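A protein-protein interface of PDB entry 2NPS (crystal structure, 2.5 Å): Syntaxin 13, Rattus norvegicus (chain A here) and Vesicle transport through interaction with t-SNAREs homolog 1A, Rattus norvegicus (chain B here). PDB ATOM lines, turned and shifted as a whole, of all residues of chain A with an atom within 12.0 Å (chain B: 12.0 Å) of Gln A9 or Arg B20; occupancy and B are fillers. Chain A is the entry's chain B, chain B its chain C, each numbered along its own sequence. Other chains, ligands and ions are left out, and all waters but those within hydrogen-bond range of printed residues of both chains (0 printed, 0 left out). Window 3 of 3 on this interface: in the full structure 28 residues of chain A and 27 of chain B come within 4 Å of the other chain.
The guanidinium group (NH2) of Arg B20 is in hydrogen-bond range of the side-chain amide oxygen (OE1) of Gln A9 (3.4 Å).
Ser B17 touches Ile A8. CG2 of Ile A8 touches CD2 of Leu B21, at 3.8 Å. CG of Glu A12 touches O of Arg B20 (3.5 Å). Ala B23 touches Glu A12. CG of Glu A12 touches CA of Gly B24 (3.97 Å). Gly B24 touches Ile A15 (O to CD1, 3.2 Å). Ile A15 touches Ile B27 (CG2 to CG2, 3.8 Å). Leu A16 touches Ile B27. Asn A19 touches Ile B27.
No residue of chain B comes within 4 Å of Thr A6. Ile A8 touches just these residues of chain B: Ser B17 and Leu B21. No residue of chain B comes within 4 Å of Gln A10. No residue of chain B comes within 4 Å of Leu A11. Of chain B, only Arg B20, Ala B23 and Gly B24 come within 4 Å of Glu A12. No residue of chain B comes within 4 Å of Ala A13. Of the printed residues of chain B, Asn A19 touches Ile B27. No residue of chain A comes within 4 Å of Ser B18. No residue of chain A comes within 4 Å of Arg B19. Arg B20 touches two residues of chain A. Leu B21 touches just one residue of chain A: Ile A8. Printed residues of chain A within 4 Å of Ala B23: Glu A12. Of the printed residues of chain A, Gly B24 touches Glu A12 and Ile A15. Tyr B25 touches none of the printed residues of chain A. Printed residues of chain A within 4 Å of Ile B27: Ile A15 (3.8 Å), Leu A16 (3.3 Å) and Asn A19 (3.5 Å). The nearest printed residue of chain B that does not touch Asn A19 is Glu B30 (4.3 Å).
Of the 22 printed residues of chain B, 6 touch a printed residue of chain A. Hydrophobic or aromatic side chains of chain B within 4 Å of the printed part of chain A: Leu B21, Ala B23 and Ile B27. Of the 19 printed residues of chain A, 6 touch a printed residue of chain B. Printed residues of chain A that touch a printed residue of chain B: Ile A8, Gln A9, Glu A12, Ile A15, Leu A16 and Asn A19. Among the printed residues, no Asp or Glu carboxylate lies within 4 Å of a Lys or Arg side-chain nitrogen of the other chain.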
ATOM      1  N   GLY A   1     -18.392  17.183 -26.337  1.00  0.00           N
ATOM      2  CA  GLY A   1     -18.696  17.632 -24.952  1.00  0.00           C
ATOM      3  C   GLY A   1     -19.344  16.533 -24.132  1.00  0.00           C
ATOM      4  O   GLY A   1     -18.851  15.406 -24.082  1.00  0.00           O
ATOM      5  N   SER A   2     -20.460  16.864 -23.494  1.00  0.00           N
ATOM      6  CA  SER A   2     -21.199  15.907 -22.683  1.00  0.00           C
ATOM      7  C   SER A   2     -22.317  15.257 -23.504  1.00  0.00           C
ATOM      8  O   SER A   2     -23.196  14.569 -22.961  1.00  0.00           O
ATOM      9  CB  SER A   2     -21.773  16.597 -21.436  1.00  0.00           C
ATOM     10  OG  SER A   2     -22.367  17.841 -21.745  1.00  0.00           O
ATOM     11  N   MET A   3     -22.266  15.479 -24.819  1.00  0.00           N
ATOM     12  CA  MET A   3     -23.236  14.914 -25.756  1.00  0.00           C
ATOM     13  C   MET A   3     -22.679  13.546 -26.144  1.00  0.00           C
ATOM     14  O   MET A   3     -23.258  12.797 -26.941  1.00  0.00           O
ATOM     15  N   ARG A   4     -21.517  13.267 -25.562  1.00  0.00           N
ATOM     16  CA  ARG A   4     -20.774  12.022 -25.720  1.00  0.00           C
ATOM     17  C   ARG A   4     -21.044  11.241 -24.433  1.00  0.00           C
ATOM     18  O   ARG A   4     -20.799  10.042 -24.348  1.00  0.00           O
ATOM     19  N   GLU A   5     -21.543  11.964 -23.433  1.00  0.00           N
ATOM     20  CA  GLU A   5     -21.886  11.409 -22.126  1.00  0.00           C
ATOM     21  C   GLU A   5     -23.318  10.874 -22.171  1.00  0.00           C
ATOM     22  O   GLU A   5     -23.625   9.819 -21.623  1.00  0.00           O
ATOM     23  CB  GLU A   5     -21.783  12.501 -21.059  1.00  0.00           C
ATOM     24  CG  GLU A   5     -22.277  12.084 -19.686  1.00  0.00           C
ATOM     25  CD  GLU A   5     -22.141  13.188 -18.647  1.00  0.00           C
ATOM     26  N   THR A   6     -24.186  11.626 -22.837  1.00  0.00           N
ATOM     27  CA  THR A   6     -25.591  11.256 -22.982  1.00  0.00           C
ATOM     28  C   THR A   6     -25.677  10.131 -24.012  1.00  0.00           C
ATOM     29  O   THR A   6     -26.351   9.123 -23.800  1.00  0.00           O
ATOM     30  CB  THR A   6     -26.417  12.465 -23.462  1.00  0.00           C
ATOM     31  N   ALA A   7     -24.954  10.310 -25.115  1.00  0.00           N
ATOM     32  CA  ALA A   7     -24.923   9.335 -26.197  1.00  0.00           C
ATOM     33  C   ALA A   7     -24.549   7.955 -25.686  1.00  0.00           C
ATOM     34  O   ALA A   7     -25.146   6.959 -26.084  1.00  0.00           O
ATOM     35  CB  ALA A   7     -23.936   9.774 -27.258  1.00  0.00           C
ATOM     36  N   ILE A   8     -23.562   7.902 -24.798  1.00  0.00           N
ATOM     37  CA  ILE A   8     -23.125   6.631 -24.233  1.00  0.00           C
ATOM     38  C   ILE A   8     -24.215   6.085 -23.333  1.00  0.00           C
ATOM     39  O   ILE A   8     -24.274   4.882 -23.073  1.00  0.00           O
ATOM     40  CB  ILE A   8     -21.822   6.778 -23.416  1.00  0.00           C
ATOM     41  CG1 ILE A   8     -20.623   6.848 -24.364  1.00  0.00           C
ATOM     42  CG2 ILE A   8     -21.663   5.606 -22.448  1.00  0.00           C
ATOM     43  N   GLN A   9     -25.083   6.967 -22.857  1.00  0.00           N
ATOM     44  CA  GLN A   9     -26.153   6.509 -21.997  1.00  0.00           C
ATOM     45  C   GLN A   9     -27.259   5.937 -22.869  1.00  0.00           C
ATOM     46  O   GLN A   9     -27.837   4.905 -22.555  1.00  0.00           O
ATOM     47  CB  GLN A   9     -26.702   7.646 -21.136  1.00  0.00           C
ATOM     48  CG  GLN A   9     -27.457   7.112 -19.930  1.00  0.00           C
ATOM     49  CD  GLN A   9     -28.242   8.163 -19.183  1.00  0.00           C
ATOM     50  OE1 GLN A   9     -27.686   9.168 -18.727  1.00  0.00           O
ATOM     51  NE2 GLN A   9     -29.546   7.930 -19.039  1.00  0.00           N
ATOM     52  N   GLN A  10     -27.544   6.618 -23.973  1.00  0.00           N
ATOM     53  CA  GLN A  10     -28.559   6.155 -24.910  1.00  0.00           C
ATOM     54  C   GLN A  10     -28.089   4.788 -25.401  1.00  0.00           C
ATOM     55  O   GLN A  10     -28.852   3.823 -25.428  1.00  0.00           O
ATOM     56  CB  GLN A  10     -28.690   7.142 -26.078  1.00  0.00           C
ATOM     57  CG  GLN A  10     -29.000   8.570 -25.598  1.00  0.00           C
ATOM     58  CD  GLN A  10     -28.950   9.621 -26.704  1.00  0.00           C
ATOM     59  OE1 GLN A  10     -28.175   9.501 -27.665  1.00  0.00           O
ATOM     60  NE2 GLN A  10     -29.758  10.674 -26.556  1.00  0.00           N
ATOM     61  N   LEU A  11     -26.814   4.711 -25.759  1.00  0.00           N
ATOM     62  CA  LEU A  11     -26.225   3.467 -26.227  1.00  0.00           C
ATOM     63  C   LEU A  11     -26.516   2.301 -25.292  1.00  0.00           C
ATOM     64  O   LEU A  11     -27.069   1.286 -25.721  1.00  0.00           O
ATOM     65  CB  LEU A  11     -24.717   3.620 -26.369  1.00  0.00           C
ATOM     66  CG  LEU A  11     -23.992   2.336 -26.744  1.00  0.00           C
ATOM     67  CD1 LEU A  11     -24.563   1.802 -28.053  1.00  0.00           C
ATOM     68  CD2 LEU A  11     -22.500   2.597 -26.869  1.00  0.00           C
ATOM     69  N   GLU A  12     -26.138   2.443 -24.024  1.00  0.00           N
ATOM     70  CA  GLU A  12     -26.352   1.385 -23.044  1.00  0.00           C
ATOM     71  C   GLU A  12     -27.836   1.107 -22.842  1.00  0.00           C
ATOM     72  O   GLU A  12     -28.252  -0.049 -22.723  1.00  0.00           O
ATOM     73  CB  GLU A  12     -25.720   1.744 -21.703  1.00  0.00           C
ATOM     74  CG  GLU A  12     -25.724   0.572 -20.742  1.00  0.00           C
ATOM     75  CD  GLU A  12     -25.671   0.988 -19.288  1.00  0.00           C
ATOM     76  OE1 GLU A  12     -26.112   2.117 -18.973  1.00  0.00           O
ATOM     77  OE2 GLU A  12     -25.213   0.172 -18.458  1.00  0.00           O
ATOM     78  N   ALA A  13     -28.629   2.171 -22.804  1.00  0.00           N
ATOM     79  CA  ALA A  13     -30.065   2.030 -22.655  1.00  0.00           C
ATOM     80  C   ALA A  13     -30.550   1.194 -23.828  1.00  0.00           C
ATOM     81  O   ALA A  13     -31.293   0.235 -23.661  1.00  0.00           O
ATOM     82  CB  ALA A  13     -30.740   3.399 -22.675  1.00  0.00           C
ATOM     83  N   ASP A  14     -30.111   1.560 -25.023  1.00  0.00           N
ATOM     84  CA  ASP A  14     -30.509   0.831 -26.208  1.00  0.00           C
ATOM     85  C   ASP A  14     -29.972  -0.596 -26.215  1.00  0.00           C
ATOM     86  O   ASP A  14     -30.599  -1.498 -26.767  1.00  0.00           O
ATOM     87  CB  ASP A  14     -30.092   1.599 -27.454  1.00  0.00           C
ATOM     88  CG  ASP A  14     -31.043   2.759 -27.753  1.00  0.00           C
ATOM     89  OD1 ASP A  14     -30.812   3.519 -28.724  1.00  0.00           O
ATOM     90  OD2 ASP A  14     -32.042   2.910 -27.006  1.00  0.00           O
ATOM     91  N   ILE A  15     -28.827  -0.818 -25.578  1.00  0.00           N
ATOM     92  CA  ILE A  15     -28.297  -2.170 -25.510  1.00  0.00           C
ATOM     93  C   ILE A  15     -29.196  -2.982 -24.591  1.00  0.00           C
ATOM     94  O   ILE A  15     -29.353  -4.186 -24.775  1.00  0.00           O
ATOM     95  CB  ILE A  15     -26.847  -2.216 -24.977  1.00  0.00           C
ATOM     96  CG1 ILE A  15     -25.878  -1.715 -26.061  1.00  0.00           C
ATOM     97  CG2 ILE A  15     -26.494  -3.645 -24.568  1.00  0.00           C
ATOM     98  CD1 ILE A  15     -24.409  -1.739 -25.644  1.00  0.00           C
ATOM     99  N   LEU A  16     -29.797  -2.327 -23.604  1.00  0.00           N
ATOM    100  CA  LEU A  16     -30.696  -3.034 -22.696  1.00  0.00           C
ATOM    101  C   LEU A  16     -31.953  -3.438 -23.442  1.00  0.00           C
ATOM    102  O   LEU A  16     -32.588  -4.435 -23.121  1.00  0.00           O
ATOM    103  CB  LEU A  16     -31.086  -2.157 -21.507  1.00  0.00           C
ATOM    104  CG  LEU A  16     -30.270  -2.405 -20.249  1.00  0.00           C
ATOM    105  CD1 LEU A  16     -30.841  -1.581 -19.102  1.00  0.00           C
ATOM    106  CD2 LEU A  16     -30.314  -3.881 -19.901  1.00  0.00           C
ATOM    107  N   ASP A  17     -32.312  -2.633 -24.434  1.00  0.00           N
ATOM    108  CA  ASP A  17     -33.485  -2.887 -25.246  1.00  0.00           C
ATOM    109  C   ASP A  17     -33.304  -4.183 -26.000  1.00  0.00           C
ATOM    110  O   ASP A  17     -34.180  -5.040 -25.971  1.00  0.00           O
ATOM    111  CB  ASP A  17     -33.702  -1.750 -26.242  1.00  0.00           C
ATOM    112  CG  ASP A  17     -34.573  -0.640 -25.677  1.00  0.00           C
ATOM    113  OD1 ASP A  17     -34.750  -0.588 -24.436  1.00  0.00           O
ATOM    114  OD2 ASP A  17     -35.075   0.192 -26.470  1.00  0.00           O
ATOM    115  N   VAL A  18     -32.166  -4.330 -26.673  1.00  0.00           N
ATOM    116  CA  VAL A  18     -31.917  -5.542 -27.428  1.00  0.00           C
ATOM    117  C   VAL A  18     -32.005  -6.717 -26.465  1.00  0.00           C
ATOM    118  O   VAL A  18     -32.709  -7.690 -26.729  1.00  0.00           O
ATOM    119  CB  VAL A  18     -30.534  -5.523 -28.137  1.00  0.00           C
ATOM    120  CG1 VAL A  18     -30.325  -4.194 -28.814  1.00  0.00           C
ATOM    121  CG2 VAL A  18     -29.412  -5.794 -27.162  1.00  0.00           C
ATOM    122  N   ASN A  19     -31.327  -6.613 -25.328  1.00  0.00           N
ATOM    123  CA  ASN A  19     -31.351  -7.697 -24.361  1.00  0.00           C
ATOM    124  C   ASN A  19     -32.779  -8.054 -24.010  1.00  0.00           C
ATOM    125  O   ASN A  19     -33.109  -9.225 -23.831  1.00  0.00           O
ATOM    126  CB  ASN A  19     -30.583  -7.322 -23.097  1.00  0.00           C
ATOM    127  CG  ASN A  19     -30.520  -8.468 -22.101  1.00  0.00           C
ATOM    128  OD1 ASN A  19     -31.419  -8.648 -21.280  1.00  0.00           O
ATOM    129  ND2 ASN A  19     -29.463  -9.264 -22.185  1.00  0.00           N
ATOM    130  N   ASP B   9     -15.452  16.857 -11.250  1.00  0.00           N
ATOM    131  CA  ASP B   9     -16.754  16.538 -11.818  1.00  0.00           C
ATOM    132  C   ASP B   9     -16.530  15.919 -13.188  1.00  0.00           C
ATOM    133  O   ASP B   9     -17.013  14.828 -13.477  1.00  0.00           O
ATOM    134  CB  ASP B   9     -17.601  17.807 -11.960  1.00  0.00           C
ATOM    135  CG  ASP B   9     -18.738  17.635 -12.948  1.00  0.00           C
ATOM    136  OD1 ASP B   9     -18.655  18.191 -14.067  1.00  0.00           O
ATOM    137  OD2 ASP B   9     -19.712  16.929 -12.613  1.00  0.00           O
ATOM    138  N   ASN B  10     -15.784  16.634 -14.023  1.00  0.00           N
ATOM    139  CA  ASN B  10     -15.474  16.181 -15.368  1.00  0.00           C
ATOM    140  C   ASN B  10     -14.825  14.798 -15.328  1.00  0.00           C
ATOM    141  O   ASN B  10     -15.101  13.967 -16.179  1.00  0.00           O
ATOM    142  CB  ASN B  10     -14.527  17.173 -16.052  1.00  0.00           C
ATOM    143  CG  ASN B  10     -14.308  16.854 -17.511  1.00  0.00           C
ATOM    144  N   THR B  11     -13.978  14.545 -14.334  1.00  0.00           N
ATOM    145  CA  THR B  11     -13.294  13.259 -14.239  1.00  0.00           C
ATOM    146  C   THR B  11     -14.185  12.113 -13.753  1.00  0.00           C
ATOM    147  O   THR B  11     -13.920  10.947 -14.054  1.00  0.00           O
ATOM    148  CB  THR B  11     -12.047  13.339 -13.317  1.00  0.00           C
ATOM    149  OG1 THR B  11     -11.004  12.513 -13.853  1.00  0.00           O
ATOM    150  CG2 THR B  11     -12.379  12.856 -11.915  1.00  0.00           C
ATOM    151  N   GLU B  12     -15.231  12.431 -12.998  1.00  0.00           N
ATOM    152  CA  GLU B  12     -16.134  11.397 -12.505  1.00  0.00           C
ATOM    153  C   GLU B  12     -17.135  11.067 -13.618  1.00  0.00           C
ATOM    154  O   GLU B  12     -17.604   9.933 -13.744  1.00  0.00           O
ATOM    155  CB  GLU B  12     -16.871  11.869 -11.240  1.00  0.00           C
ATOM    156  N   ARG B  13     -17.456  12.073 -14.427  1.00  0.00           N
ATOM    157  CA  ARG B  13     -18.378  11.901 -15.545  1.00  0.00           C
ATOM    158  C   ARG B  13     -17.764  10.904 -16.515  1.00  0.00           C
ATOM    159  O   ARG B  13     -18.472  10.232 -17.257  1.00  0.00           O
ATOM    160  CB  ARG B  13     -18.615  13.245 -16.254  1.00  0.00           C
ATOM    161  N   LEU B  14     -16.439  10.815 -16.496  1.00  0.00           N
ATOM    162  CA  LEU B  14     -15.707   9.893 -17.360  1.00  0.00           C
ATOM    163  C   LEU B  14     -15.693   8.499 -16.753  1.00  0.00           C
ATOM    164  O   LEU B  14     -15.925   7.514 -17.445  1.00  0.00           O
ATOM    165  CB  LEU B  14     -14.261  10.367 -17.545  1.00  0.00           C
ATOM    166  CG  LEU B  14     -13.880  11.185 -18.774  1.00  0.00           C
ATOM    167  N   GLU B  15     -15.406   8.429 -15.458  1.00  0.00           N
ATOM    168  CA  GLU B  15     -15.331   7.157 -14.746  1.00  0.00           C
ATOM    169  C   GLU B  15     -16.557   6.258 -14.894  1.00  0.00           C
ATOM    170  O   GLU B  15     -16.431   5.086 -15.257  1.00  0.00           O
ATOM    171  N   ARG B  16     -17.736   6.810 -14.618  1.00  0.00           N
ATOM    172  CA  ARG B  16     -18.980   6.054 -14.707  1.00  0.00           C
ATOM    173  C   ARG B  16     -19.398   5.835 -16.161  1.00  0.00           C
ATOM    174  O   ARG B  16     -20.150   4.908 -16.479  1.00  0.00           O
ATOM    175  CB  ARG B  16     -20.085   6.779 -13.932  1.00  0.00           C
ATOM    176  CG  ARG B  16     -20.127   8.274 -14.188  1.00  0.00           C
ATOM    177  CD  ARG B  16     -21.246   8.697 -15.137  1.00  0.00           C
ATOM    178  NE  ARG B  16     -22.520   8.873 -14.438  1.00  0.00           N
ATOM    179  CZ  ARG B  16     -23.447   9.771 -14.772  1.00  0.00           C
ATOM    180  NH1 ARG B  16     -24.578   9.855 -14.073  1.00  0.00           N
ATOM    181  NH2 ARG B  16     -23.247  10.594 -15.797  1.00  0.00           N
ATOM    182  N   SER B  17     -18.904   6.681 -17.052  1.00  0.00           N
ATOM    183  CA  SER B  17     -19.237   6.525 -18.457  1.00  0.00           C
ATOM    184  C   SER B  17     -18.483   5.301 -18.958  1.00  0.00           C
ATOM    185  O   SER B  17     -18.861   4.673 -19.937  1.00  0.00           O
ATOM    186  CB  SER B  17     -18.817   7.758 -19.259  1.00  0.00           C
ATOM    187  OG  SER B  17     -19.280   7.670 -20.595  1.00  0.00           O
ATOM    188  N   SER B  18     -17.402   4.972 -18.268  1.00  0.00           N
ATOM    189  CA  SER B  18     -16.588   3.823 -18.625  1.00  0.00           C
ATOM    190  C   SER B  18     -17.258   2.609 -18.025  1.00  0.00           C
ATOM    191  O   SER B  18     -17.082   1.497 -18.504  1.00  0.00           O
ATOM    192  CB  SER B  18     -15.171   3.965 -18.052  1.00  0.00           C
ATOM    193  OG  SER B  18     -14.346   2.893 -18.482  1.00  0.00           O
ATOM    194  N   ARG B  19     -18.023   2.839 -16.961  1.00  0.00           N
ATOM    195  CA  ARG B  19     -18.746   1.777 -16.263  1.00  0.00           C
ATOM    196  C   ARG B  19     -20.098   1.542 -16.926  1.00  0.00           C
ATOM    197  O   ARG B  19     -20.871   0.689 -16.504  1.00  0.00           O
ATOM    198  N   ARG B  20     -20.376   2.320 -17.965  1.00  0.00           N
ATOM    199  CA  ARG B  20     -21.619   2.186 -18.710  1.00  0.00           C
ATOM    200  C   ARG B  20     -21.331   1.444 -20.010  1.00  0.00           C
ATOM    201  O   ARG B  20     -22.228   0.876 -20.632  1.00  0.00           O
ATOM    202  CB  ARG B  20     -22.224   3.561 -18.985  1.00  0.00           C
ATOM    203  CG  ARG B  20     -23.050   4.075 -17.825  1.00  0.00           C
ATOM    204  CD  ARG B  20     -23.571   5.473 -18.071  1.00  0.00           C
ATOM    205  NE  ARG B  20     -24.623   5.823 -17.121  1.00  0.00           N
ATOM    206  CZ  ARG B  20     -25.102   7.056 -16.952  1.00  0.00           C
ATOM    207  NH1 ARG B  20     -26.070   7.288 -16.061  1.00  0.00           N
ATOM    208  NH2 ARG B  20     -24.602   8.063 -17.664  1.00  0.00           N
ATOM    209  N   LEU B  21     -20.059   1.448 -20.395  1.00  0.00           N
ATOM    210  CA  LEU B  21     -19.580   0.753 -21.585  1.00  0.00           C
ATOM    211  C   LEU B  21     -19.109  -0.623 -21.135  1.00  0.00           C
ATOM    212  O   LEU B  21     -18.893  -1.527 -21.942  1.00  0.00           O
ATOM    213  CB  LEU B  21     -18.406   1.499 -22.203  1.00  0.00           C
ATOM    214  CG  LEU B  21     -18.699   2.876 -22.781  1.00  0.00           C
ATOM    215  CD1 LEU B  21     -17.401   3.501 -23.270  1.00  0.00           C
ATOM    216  CD2 LEU B  21     -19.703   2.744 -23.926  1.00  0.00           C
ATOM    217  N   GLU B  22     -18.918  -0.772 -19.834  1.00  0.00           N
ATOM    218  CA  GLU B  22     -18.503  -2.057 -19.317  1.00  0.00           C
ATOM    219  C   GLU B  22     -19.795  -2.833 -19.138  1.00  0.00           C
ATOM    220  O   GLU B  22     -19.864  -4.014 -19.431  1.00  0.00           O
ATOM    221  CB  GLU B  22     -17.770  -1.906 -17.983  1.00  0.00           C
ATOM    222  N   ALA B  23     -20.831  -2.153 -18.670  1.00  0.00           N
ATOM    223  CA  ALA B  23     -22.113  -2.803 -18.484  1.00  0.00           C
ATOM    224  C   ALA B  23     -22.700  -3.073 -19.853  1.00  0.00           C
ATOM    225  O   ALA B  23     -23.154  -4.174 -20.136  1.00  0.00           O
ATOM    226  CB  ALA B  23     -23.051  -1.914 -17.665  1.00  0.00           C
ATOM    227  N   GLY B  24     -22.659  -2.060 -20.711  1.00  0.00           N
ATOM    228  CA  GLY B  24     -23.191  -2.193 -22.055  1.00  0.00           C
ATOM    229  C   GLY B  24     -22.592  -3.364 -22.793  1.00  0.00           C
ATOM    230  O   GLY B  24     -23.198  -3.932 -23.693  1.00  0.00           O
ATOM    231  N   TYR B  25     -21.389  -3.731 -22.394  1.00  0.00           N
ATOM    232  CA  TYR B  25     -20.690  -4.845 -23.004  1.00  0.00           C
ATOM    233  C   TYR B  25     -21.161  -6.153 -22.370  1.00  0.00           C
ATOM    234  O   TYR B  25     -21.458  -7.125 -23.069  1.00  0.00           O
ATOM    235  CB  TYR B  25     -19.187  -4.675 -22.802  1.00  0.00           C
ATOM    236  CG  TYR B  25     -18.392  -5.883 -23.216  1.00  0.00           C
ATOM    237  CD1 TYR B  25     -18.154  -6.158 -24.564  1.00  0.00           C
ATOM    238  CD2 TYR B  25     -17.893  -6.762 -22.259  1.00  0.00           C
ATOM    239  CE1 TYR B  25     -17.449  -7.291 -24.949  1.00  0.00           C
ATOM    240  CE2 TYR B  25     -17.187  -7.897 -22.628  1.00  0.00           C
ATOM    241  CZ  TYR B  25     -16.962  -8.156 -23.974  1.00  0.00           C
ATOM    242  OH  TYR B  25     -16.273  -9.291 -24.344  1.00  0.00           O
ATOM    243  N   GLN B  26     -21.240  -6.169 -21.045  1.00  0.00           N
ATOM    244  CA  GLN B  26     -21.673  -7.362 -20.333  1.00  0.00           C
ATOM    245  C   GLN B  26     -23.072  -7.781 -20.787  1.00  0.00           C
ATOM    246  O   GLN B  26     -23.338  -8.958 -21.021  1.00  0.00           O
ATOM    247  CB  GLN B  26     -21.658  -7.110 -18.821  1.00  0.00           C
ATOM    248  N   ILE B  27     -23.964  -6.806 -20.913  1.00  0.00           N
ATOM    249  CA  ILE B  27     -25.327  -7.077 -21.332  1.00  0.00           C
ATOM    250  C   ILE B  27     -25.352  -7.708 -22.726  1.00  0.00           C
ATOM    251  O   ILE B  27     -26.033  -8.709 -22.951  1.00  0.00           O
ATOM    252  CB  ILE B  27     -26.158  -5.789 -21.337  1.00  0.00           C
ATOM    253  CG1 ILE B  27     -26.297  -5.258 -19.918  1.00  0.00           C
ATOM    254  CG2 ILE B  27     -27.531  -6.061 -21.890  1.00  0.00           C
ATOM    255  CD1 ILE B  27     -26.976  -3.917 -19.856  1.00  0.00           C
ATOM    256  N   ALA B  28     -24.607  -7.117 -23.656  1.00  0.00           N
ATOM    257  CA  ALA B  28     -24.556  -7.625 -25.016  1.00  0.00           C
ATOM    258  C   ALA B  28     -24.096  -9.072 -24.994  1.00  0.00           C
ATOM    259  O   ALA B  28     -24.806  -9.964 -25.443  1.00  0.00           O
ATOM    260  CB  ALA B  28     -23.615  -6.782 -25.858  1.00  0.00           C
ATOM    261  N   VAL B  29     -22.907  -9.308 -24.460  1.00  0.00           N
ATOM    262  CA  VAL B  29     -22.389 -10.667 -24.385  1.00  0.00           C
ATOM    263  C   VAL B  29     -23.440 -11.601 -23.799  1.00  0.00           C
ATOM    264  O   VAL B  29     -23.626 -12.715 -24.295  1.00  0.00           O
ATOM    265  CB  VAL B  29     -21.116 -10.749 -23.512  1.00  0.00           C
ATOM    266  CG1 VAL B  29     -20.754 -12.210 -23.244  1.00  0.00           C
ATOM    267  CG2 VAL B  29     -19.973 -10.035 -24.211  1.00  0.00           C
ATOM    268  N   GLU B  30     -24.123 -11.155 -22.746  1.00  0.00           N
ATOM    269  CA  GLU B  30     -25.160 -11.978 -22.140  1.00  0.00           C
ATOM    270  C   GLU B  30     -26.177 -12.284 -23.235  1.00  0.00           C
ATOM    271  O   GLU B  30     -26.513 -13.447 -23.467  1.00  0.00           O
ATOM    272  CB  GLU B  30     -25.836 -11.258 -20.952  1.00  0.00           C
ATOM    273  CG  GLU B  30     -25.202 -11.592 -19.590  1.00  0.00           C
ATOM    274  CD  GLU B  30     -25.723 -10.747 -18.414  1.00  0.00           C
ATOM    275  OE1 GLU B  30     -26.351  -9.690 -18.645  1.00  0.00           O
ATOM    276  OE2 GLU B  30     -25.474 -11.137 -17.243  1.00  0.00           O
